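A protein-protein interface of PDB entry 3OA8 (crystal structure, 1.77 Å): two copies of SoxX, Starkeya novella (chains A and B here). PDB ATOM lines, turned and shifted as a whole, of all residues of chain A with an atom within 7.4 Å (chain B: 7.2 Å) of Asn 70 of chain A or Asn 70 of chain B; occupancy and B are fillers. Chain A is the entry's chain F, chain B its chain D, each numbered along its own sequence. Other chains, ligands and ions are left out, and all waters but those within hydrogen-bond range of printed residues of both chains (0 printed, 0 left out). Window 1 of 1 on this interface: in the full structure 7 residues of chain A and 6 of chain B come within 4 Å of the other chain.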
ATOM      1  N   ILE A  63       6.692 -23.908 -20.705  1.00  0.00           N
ATOM      2  CA  ILE A  63       5.403 -23.193 -20.755  1.00  0.00           C
ATOM      3  C   ILE A  63       4.557 -23.670 -21.916  1.00  0.00           C
ATOM      4  O   ILE A  63       3.346 -23.917 -21.755  1.00  0.00           O
ATOM      5  CB  ILE A  63       5.606 -21.653 -20.845  1.00  0.00           C
ATOM      6  CG1 ILE A  63       6.273 -21.117 -19.566  1.00  0.00           C
ATOM      7  CG2 ILE A  63       4.275 -20.946 -20.988  1.00  0.00           C
ATOM      8  CD1 ILE A  63       6.912 -19.753 -19.737  1.00  0.00           C
ATOM      9  N   CYS A  64       5.179 -23.793 -23.085  1.00  0.00           N
ATOM     10  CA  CYS A  64       4.493 -24.367 -24.255  1.00  0.00           C
ATOM     11  C   CYS A  64       4.018 -25.799 -24.026  1.00  0.00           C
ATOM     12  O   CYS A  64       2.965 -26.165 -24.499  1.00  0.00           O
ATOM     13  CB  CYS A  64       5.380 -24.287 -25.474  1.00  0.00           C
ATOM     14  SG  CYS A  64       5.670 -22.537 -25.930  1.00  0.00           S
ATOM     15  N   SER A  65       4.788 -26.599 -23.296  1.00  0.00           N
ATOM     16  CA  SER A  65       4.351 -27.955 -22.984  1.00  0.00           C
ATOM     17  C   SER A  65       3.113 -27.982 -22.076  1.00  0.00           C
ATOM     18  O   SER A  65       2.098 -28.605 -22.407  1.00  0.00           O
ATOM     19  CB  SER A  65       5.488 -28.723 -22.309  1.00  0.00           C
ATOM     20  OG  SER A  65       6.654 -28.764 -23.113  1.00  0.00           O
ATOM     21  N   VAL A  66       3.183 -27.283 -20.945  1.00  0.00           N
ATOM     22  CA  VAL A  66       2.075 -27.332 -19.993  1.00  0.00           C
ATOM     23  C   VAL A  66       0.771 -26.708 -20.552  1.00  0.00           C
ATOM     24  O   VAL A  66      -0.331 -27.117 -20.172  1.00  0.00           O
ATOM     25  CB  VAL A  66       2.470 -26.738 -18.646  1.00  0.00           C
ATOM     26  CG1 VAL A  66       3.662 -27.509 -18.038  1.00  0.00           C
ATOM     27  CG2 VAL A  66       2.775 -25.237 -18.756  1.00  0.00           C
ATOM     28  N   THR A  67       0.892 -25.760 -21.472  1.00  0.00           N
ATOM     29  CA  THR A  67      -0.292 -25.130 -22.071  1.00  0.00           C
ATOM     30  C   THR A  67      -0.706 -25.802 -23.394  1.00  0.00           C
ATOM     31  O   THR A  67      -1.620 -25.335 -24.107  1.00  0.00           O
ATOM     32  CB  THR A  67      -0.074 -23.619 -22.298  1.00  0.00           C
ATOM     33  OG1 THR A  67       1.047 -23.432 -23.166  1.00  0.00           O
ATOM     34  CG2 THR A  67       0.185 -22.864 -20.954  1.00  0.00           C
ATOM     35  N   ARG A  68      -0.062 -26.915 -23.730  1.00  0.00           N
ATOM     36  CA  ARG A  68      -0.306 -27.568 -25.034  1.00  0.00           C
ATOM     37  C   ARG A  68      -0.247 -26.601 -26.212  1.00  0.00           C
ATOM     38  O   ARG A  68      -1.129 -26.616 -27.094  1.00  0.00           O
ATOM     39  CB  ARG A  68      -1.651 -28.288 -25.005  1.00  0.00           C
ATOM     40  CG  ARG A  68      -1.692 -29.274 -23.886  1.00  0.00           C
ATOM     41  CD  ARG A  68      -3.029 -29.953 -23.774  1.00  0.00           C
ATOM     42  NE  ARG A  68      -2.909 -30.852 -22.647  1.00  0.00           N
ATOM     43  CZ  ARG A  68      -3.503 -32.030 -22.545  1.00  0.00           C
ATOM     44  NH1 ARG A  68      -4.303 -32.475 -23.511  1.00  0.00           N
ATOM     45  NH2 ARG A  68      -3.289 -32.760 -21.461  1.00  0.00           N
ATOM     46  N   ASN A  69       0.783 -25.768 -26.214  1.00  0.00           N
ATOM     47  CA  ASN A  69       1.008 -24.703 -27.203  1.00  0.00           C
ATOM     48  C   ASN A  69      -0.082 -23.637 -27.307  1.00  0.00           C
ATOM     49  O   ASN A  69      -0.096 -22.905 -28.287  1.00  0.00           O
ATOM     50  CB  ASN A  69       1.341 -25.257 -28.611  1.00  0.00           C
ATOM     51  CG  ASN A  69       2.683 -25.965 -28.666  1.00  0.00           C
ATOM     52  OD1 ASN A  69       3.563 -25.764 -27.816  1.00  0.00           O
ATOM     53  ND2 ASN A  69       2.863 -26.776 -29.714  1.00  0.00           N
ATOM     54  N   ASN A  70      -0.952 -23.521 -26.296  1.00  0.00           N
ATOM     55  CA  ASN A  70      -1.942 -22.479 -26.261  1.00  0.00           C
ATOM     56  C   ASN A  70      -1.772 -21.653 -24.991  1.00  0.00           C
ATOM     57  O   ASN A  70      -2.611 -21.732 -24.080  1.00  0.00           O
ATOM     58  CB  ASN A  70      -3.377 -23.033 -26.335  1.00  0.00           C
ATOM     59  CG  ASN A  70      -4.379 -21.967 -26.682  1.00  0.00           C
ATOM     60  OD1 ASN A  70      -4.055 -20.771 -26.713  1.00  0.00           O
ATOM     61  ND2 ASN A  70      -5.601 -22.395 -27.014  1.00  0.00           N
ATOM     62  N   PRO A  71      -0.717 -20.814 -24.938  1.00  0.00           N
ATOM     63  CA  PRO A  71      -0.490 -19.954 -23.755  1.00  0.00           C
ATOM     64  C   PRO A  71      -1.550 -18.889 -23.606  1.00  0.00           C
ATOM     65  O   PRO A  71      -2.179 -18.507 -24.593  1.00  0.00           O
ATOM     66  CB  PRO A  71       0.854 -19.295 -24.029  1.00  0.00           C
ATOM     67  CG  PRO A  71       1.015 -19.320 -25.503  1.00  0.00           C
ATOM     68  CD  PRO A  71       0.291 -20.593 -25.988  1.00  0.00           C
ATOM     69  N   SER A  72      -1.750 -18.406 -22.381  1.00  0.00           N
ATOM     70  CA  SER A  72      -2.671 -17.297 -22.127  1.00  0.00           C
ATOM     71  C   SER A  72      -2.084 -16.026 -22.777  1.00  0.00           C
ATOM     72  O   SER A  72      -0.878 -16.018 -23.083  1.00  0.00           O
ATOM     73  CB  SER A  72      -2.787 -17.058 -20.628  1.00  0.00           C
ATOM     74  OG  SER A  72      -1.542 -16.573 -20.130  1.00  0.00           O
ATOM     75  N   PRO A  73      -2.902 -14.963 -22.985  1.00  0.00           N
ATOM     76  CA  PRO A  73      -2.326 -13.706 -23.509  1.00  0.00           C
ATOM     77  C   PRO A  73      -1.069 -13.271 -22.731  1.00  0.00           C
ATOM     78  O   PRO A  73      -0.053 -12.877 -23.323  1.00  0.00           O
ATOM     79  CB  PRO A  73      -3.488 -12.701 -23.329  1.00  0.00           C
ATOM     80  CG  PRO A  73      -4.696 -13.566 -23.567  1.00  0.00           C
ATOM     81  CD  PRO A  73      -4.373 -14.866 -22.858  1.00  0.00           C
ATOM     82  N   GLN A  75       1.050 -15.144 -20.867  1.00  0.00           N
ATOM     83  CA  GLN A  75       2.197 -16.043 -21.098  1.00  0.00           C
ATOM     84  C   GLN A  75       2.775 -15.844 -22.499  1.00  0.00           C
ATOM     85  O   GLN A  75       3.990 -15.929 -22.674  1.00  0.00           O
ATOM     86  CB  GLN A  75       1.806 -17.504 -20.894  1.00  0.00           C
ATOM     87  CG  GLN A  75       1.289 -17.827 -19.498  1.00  0.00           C
ATOM     88  CD  GLN A  75       0.682 -19.223 -19.437  1.00  0.00           C
ATOM     89  OE1 GLN A  75      -0.164 -19.579 -20.261  1.00  0.00           O
ATOM     90  NE2 GLN A  75       1.131 -20.031 -18.467  1.00  0.00           N
ATOM     91  N   ALA A  76       1.910 -15.637 -23.500  1.00  0.00           N
ATOM     92  CA  ALA A  76       2.355 -15.437 -24.877  1.00  0.00           C
ATOM     93  C   ALA A  76       3.242 -14.201 -24.969  1.00  0.00           C
ATOM     94  O   ALA A  76       4.336 -14.231 -25.585  1.00  0.00           O
ATOM     95  CB  ALA A  76       1.140 -15.280 -25.792  1.00  0.00           C
ATOM     96  N   ALA A 174       4.091 -17.093 -30.322  1.00  0.00           N
ATOM     97  CA  ALA A 174       4.288 -17.883 -29.118  1.00  0.00           C
ATOM     98  C   ALA A 174       3.884 -19.342 -29.327  1.00  0.00           C
ATOM     99  O   ALA A 174       2.802 -19.625 -29.877  1.00  0.00           O
ATOM    100  CB  ALA A 174       3.494 -17.239 -27.924  1.00  0.00           C
ATOM    101  N   CYS A 175       4.800 -20.254 -28.961  1.00  0.00           N
ATOM    102  CA  CYS A 175       4.594 -21.712 -29.027  1.00  0.00           C
ATOM    103  C   CYS A 175       4.448 -22.256 -30.465  1.00  0.00           C
ATOM    104  O   CYS A 175       3.886 -23.317 -30.679  1.00  0.00           O
ATOM    105  CB  CYS A 175       3.467 -22.180 -28.086  1.00  0.00           C
ATOM    106  SG  CYS A 175       3.812 -21.762 -26.345  1.00  0.00           S
ATOM    107  N   ILE B  63     -11.912 -27.260 -36.509  1.00  0.00           N
ATOM    108  CA  ILE B  63     -10.925 -26.766 -35.535  1.00  0.00           C
ATOM    109  C   ILE B  63     -11.599 -25.930 -34.467  1.00  0.00           C
ATOM    110  O   ILE B  63     -11.251 -26.020 -33.279  1.00  0.00           O
ATOM    111  CB  ILE B  63      -9.784 -25.942 -36.180  1.00  0.00           C
ATOM    112  CG1 ILE B  63      -8.924 -26.838 -37.080  1.00  0.00           C
ATOM    113  CG2 ILE B  63      -8.894 -25.313 -35.053  1.00  0.00           C
ATOM    114  CD1 ILE B  63      -7.935 -26.053 -37.983  1.00  0.00           C
ATOM    115  N   CYS B  64     -12.542 -25.079 -34.876  1.00  0.00           N
ATOM    116  CA  CYS B  64     -13.227 -24.238 -33.887  1.00  0.00           C
ATOM    117  C   CYS B  64     -14.064 -25.086 -32.963  1.00  0.00           C
ATOM    118  O   CYS B  64     -14.235 -24.732 -31.814  1.00  0.00           O
ATOM    119  CB  CYS B  64     -14.065 -23.180 -34.562  1.00  0.00           C
ATOM    120  SG  CYS B  64     -12.975 -22.006 -35.452  1.00  0.00           S
ATOM    121  N   SER B  65     -14.574 -26.213 -33.458  1.00  0.00           N
ATOM    122  CA  SER B  65     -15.274 -27.121 -32.540  1.00  0.00           C
ATOM    123  C   SER B  65     -14.332 -27.763 -31.492  1.00  0.00           C
ATOM    124  O   SER B  65     -14.594 -27.707 -30.291  1.00  0.00           O
ATOM    125  CB  SER B  65     -16.013 -28.169 -33.334  1.00  0.00           C
ATOM    126  OG  SER B  65     -16.958 -27.534 -34.202  1.00  0.00           O
ATOM    127  N   VAL B  66     -13.246 -28.338 -31.963  1.00  0.00           N
ATOM    128  CA  VAL B  66     -12.342 -29.110 -31.119  1.00  0.00           C
ATOM    129  C   VAL B  66     -11.734 -28.191 -30.060  1.00  0.00           C
ATOM    130  O   VAL B  66     -11.575 -28.597 -28.902  1.00  0.00           O
ATOM    131  CB  VAL B  66     -11.241 -29.777 -31.932  1.00  0.00           C
ATOM    132  CG1 VAL B  66     -10.122 -30.302 -30.996  1.00  0.00           C
ATOM    133  CG2 VAL B  66     -11.808 -30.923 -32.823  1.00  0.00           C
ATOM    134  N   THR B  67     -11.405 -26.949 -30.453  1.00  0.00           N
ATOM    135  CA  THR B  67     -10.741 -26.019 -29.540  1.00  0.00           C
ATOM    136  C   THR B  67     -11.716 -25.145 -28.774  1.00  0.00           C
ATOM    137  O   THR B  67     -11.295 -24.229 -28.025  1.00  0.00           O
ATOM    138  CB  THR B  67      -9.772 -25.047 -30.267  1.00  0.00           C
ATOM    139  OG1 THR B  67     -10.536 -24.218 -31.133  1.00  0.00           O
ATOM    140  CG2 THR B  67      -8.711 -25.753 -31.048  1.00  0.00           C
ATOM    141  N   ARG B  68     -13.009 -25.381 -28.990  1.00  0.00           N
ATOM    142  CA  ARG B  68     -14.092 -24.601 -28.326  1.00  0.00           C
ATOM    143  C   ARG B  68     -13.868 -23.106 -28.543  1.00  0.00           C
ATOM    144  O   ARG B  68     -13.909 -22.308 -27.594  1.00  0.00           O
ATOM    145  CB  ARG B  68     -14.109 -24.927 -26.823  1.00  0.00           C
ATOM    146  CG  ARG B  68     -14.048 -26.445 -26.537  1.00  0.00           C
ATOM    147  CD  ARG B  68     -15.436 -26.964 -26.405  1.00  0.00           C
ATOM    148  NE  ARG B  68     -15.622 -28.408 -26.560  1.00  0.00           N
ATOM    149  CZ  ARG B  68     -15.966 -29.245 -25.596  1.00  0.00           C
ATOM    150  NH1 ARG B  68     -16.121 -28.817 -24.341  1.00  0.00           N
ATOM    151  NH2 ARG B  68     -16.143 -30.525 -25.891  1.00  0.00           N
ATOM    152  N   ASN B  69     -13.575 -22.756 -29.792  1.00  0.00           N
ATOM    153  CA  ASN B  69     -13.389 -21.374 -30.257  1.00  0.00           C
ATOM    154  C   ASN B  69     -12.150 -20.702 -29.672  1.00  0.00           C
ATOM    155  O   ASN B  69     -11.967 -19.487 -29.837  1.00  0.00           O
ATOM    156  CB  ASN B  69     -14.639 -20.501 -30.029  1.00  0.00           C
ATOM    157  CG  ASN B  69     -15.808 -20.834 -30.993  1.00  0.00           C
ATOM    158  OD1 ASN B  69     -15.645 -21.530 -31.996  1.00  0.00           O
ATOM    159  ND2 ASN B  69     -16.995 -20.275 -30.689  1.00  0.00           N
ATOM    160  N   ASN B  70     -11.270 -21.496 -29.075  1.00  0.00           N
ATOM    161  CA  ASN B  70     -10.030 -20.939 -28.553  1.00  0.00           C
ATOM    162  C   ASN B  70      -8.795 -21.614 -29.169  1.00  0.00           C
ATOM    163  O   ASN B  70      -8.047 -22.336 -28.465  1.00  0.00           O
ATOM    164  CB  ASN B  70      -9.997 -21.045 -27.050  1.00  0.00           C
ATOM    165  CG  ASN B  70      -8.874 -20.239 -26.434  1.00  0.00           C
ATOM    166  OD1 ASN B  70      -8.115 -19.536 -27.114  1.00  0.00           O
ATOM    167  ND2 ASN B  70      -8.766 -20.328 -25.141  1.00  0.00           N
ATOM    168  N   PRO B  71      -8.531 -21.342 -30.457  1.00  0.00           N
ATOM    169  CA  PRO B  71      -7.320 -21.941 -31.059  1.00  0.00           C
ATOM    170  C   PRO B  71      -6.029 -21.357 -30.521  1.00  0.00           C
ATOM    171  O   PRO B  71      -6.010 -20.212 -30.048  1.00  0.00           O
ATOM    172  CB  PRO B  71      -7.470 -21.605 -32.553  1.00  0.00           C
ATOM    173  CG  PRO B  71      -8.271 -20.362 -32.595  1.00  0.00           C
ATOM    174  CD  PRO B  71      -9.270 -20.490 -31.417  1.00  0.00           C
ATOM    175  N   SER B  72      -4.950 -22.124 -30.633  1.00  0.00           N
ATOM    176  CA  SER B  72      -3.598 -21.684 -30.261  1.00  0.00           C
ATOM    177  C   SER B  72      -3.182 -20.537 -31.175  1.00  0.00           C
ATOM    178  O   SER B  72      -3.800 -20.361 -32.233  1.00  0.00           O
ATOM    179  CB  SER B  72      -2.627 -22.850 -30.398  1.00  0.00           C
ATOM    180  OG  SER B  72      -2.316 -23.110 -31.763  1.00  0.00           O
ATOM    181  N   PRO B  73      -2.190 -19.731 -30.769  1.00  0.00           N
ATOM    182  CA  PRO B  73      -1.720 -18.678 -31.661  1.00  0.00           C
ATOM    183  C   PRO B  73      -1.387 -19.246 -33.065  1.00  0.00           C
ATOM    184  O   PRO B  73      -1.724 -18.616 -34.062  1.00  0.00           O
ATOM    185  CB  PRO B  73      -0.456 -18.161 -30.961  1.00  0.00           C
ATOM    186  CG  PRO B  73      -0.711 -18.346 -29.570  1.00  0.00           C
ATOM    187  CD  PRO B  73      -1.482 -19.685 -29.469  1.00  0.00           C
ATOM    188  N   GLN B  75      -2.631 -22.014 -34.575  1.00  0.00           N
ATOM    189  CA  GLN B  75      -3.868 -22.422 -35.236  1.00  0.00           C
ATOM    190  C   GLN B  75      -4.652 -21.230 -35.696  1.00  0.00           C
ATOM    191  O   GLN B  75      -5.224 -21.237 -36.790  1.00  0.00           O
ATOM    192  CB  GLN B  75      -4.724 -23.283 -34.324  1.00  0.00           C
ATOM    193  CG  GLN B  75      -4.138 -24.664 -33.997  1.00  0.00           C
ATOM    194  CD  GLN B  75      -4.981 -25.383 -32.940  1.00  0.00           C
ATOM    195  OE1 GLN B  75      -5.358 -24.799 -31.916  1.00  0.00           O
ATOM    196  NE2 GLN B  75      -5.345 -26.642 -33.219  1.00  0.00           N
ATOM    197  N   ALA B  76      -4.732 -20.211 -34.848  1.00  0.00           N
ATOM    198  CA  ALA B  76      -5.428 -18.956 -35.229  1.00  0.00           C
ATOM    199  C   ALA B  76      -4.815 -18.312 -36.473  1.00  0.00           C
ATOM    200  O   ALA B  76      -5.536 -17.852 -37.343  1.00  0.00           O
ATOM    201  CB  ALA B  76      -5.452 -17.965 -34.061  1.00  0.00           C
ATOM    202  N   ALA B 174     -10.042 -15.366 -35.539  1.00  0.00           N
ATOM    203  CA  ALA B 174     -10.214 -16.824 -35.655  1.00  0.00           C
ATOM    204  C   ALA B 174     -11.332 -17.316 -34.766  1.00  0.00           C
ATOM    205  O   ALA B 174     -11.399 -16.925 -33.631  1.00  0.00           O
ATOM    206  CB  ALA B 174      -8.893 -17.564 -35.299  1.00  0.00           C
ATOM    207  N   CYS B 175     -12.211 -18.149 -35.311  1.00  0.00           N
ATOM    208  CA  CYS B 175     -13.318 -18.772 -34.570  1.00  0.00           C
ATOM    209  C   CYS B 175     -14.369 -17.771 -34.057  1.00  0.00           C
ATOM    210  O   CYS B 175     -15.158 -18.110 -33.154  1.00  0.00           O
ATOM    211  CB  CYS B 175     -12.819 -19.700 -33.443  1.00  0.00           C
ATOM    212  SG  CYS B 175     -11.802 -21.070 -34.056  1.00  0.00           S
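ND2 of Asn 70 of chain A is in hydrogen-bond range of O of Asn 70 of chain B (2.8 Å).
The side-chain hydroxyl (OG1) of Thr 67 of chain B is in hydrogen-bond range of the backbone NH (N) of Asn 70 of chain B (3.5 Å).
N of Ser 72 of chain B lies within hydrogen-bond range of OE1 of Gln 75 of chain B (3.0 Å).
The backbone carbonyl oxygen of Cys 64 of chain A is in hydrogen-bond range of the backbone NH of Asn 69 of chain A, at 2.8 Å.
SG of Cys 64 of chain B is disulfide-bonded to SG of Cys 175 of chain B, at 2.0 Å.
The side-chain sulfur (SG) of Cys 64 of chain A forms a disulfide with the side-chain sulfur (SG) of Cys 175 of chain A, at 2.1 Å.
Asn 69 of chain A touches Ser 72 of chain B.
Asn 69 of chain A touches Pro 73 of chain B.
C of Pro 71 of chain B touches ND2 of Asn 70 of chain A, 3.7 Å away.
Asn 70 of chain A touches Ser 72 of chain B (CG to CA, 3.7 Å).
Pro 73 of chain B touches Asn 70 of chain A (CD to OD1, 3.9 Å).
Ala 174 of chain A touches Pro 73 of chain B (O to CB, 3.7 Å).
Asn 70 of chain A touches four residues of chain B.
Of the printed residues of chain A, Asn 70 of chain B touches Asn 70.
Of the printed residues of chain A, Pro 73 of chain B touches Asn 69 (3.7 Å), Asn 70 (3.9 Å) and Ala 174 (3.7 Å).
Printed residues of chain A within 4 Å of Pro 71 of chain B: Asn 70.
Thr 67 of chain A touches none of the printed residues of chain B.
Ala 76 of chain A touches none of the printed residues of chain B.
The nearest residue of chain B that does not touch Asn 70 of chain A is Gln 75 of chain B (5.5 Å).
The nearest residue of chain A that does not touch Asn 70 of chain B is Pro 71 of chain A (6.5 Å).
Hydrophobic or aromatic side chains of chain B that line the printed part of chain A: Pro 73.
Among the printed residues, 7 pairs touch across the chains.
Asn 69 of chain A touches Ser 72 of chain B, but with the chains exchanged Ser 72 of chain A does not touch Asn 69 of chain B (12.3 Å).
Asn 70 of chain A touches Pro 71 of chain B, but with the chains exchanged Pro 71 of chain A does not touch Asn 70 of chain B (6.5 Å).
Asn 70 of chain A touches Pro 73 of chain B, but with the chains exchanged Pro 73 of chain A does not touch Asn 70 of chain B (7.3 Å).
Ala 174 of chain A touches Pro 73 of chain B, but with the chains exchanged Pro 73 of chain A does not touch Ala 174 of chain B (12.5 Å).
Of the 7 pairs that touch across the chains among the printed residues, 1 has its exchanged pair printed and touching as well.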
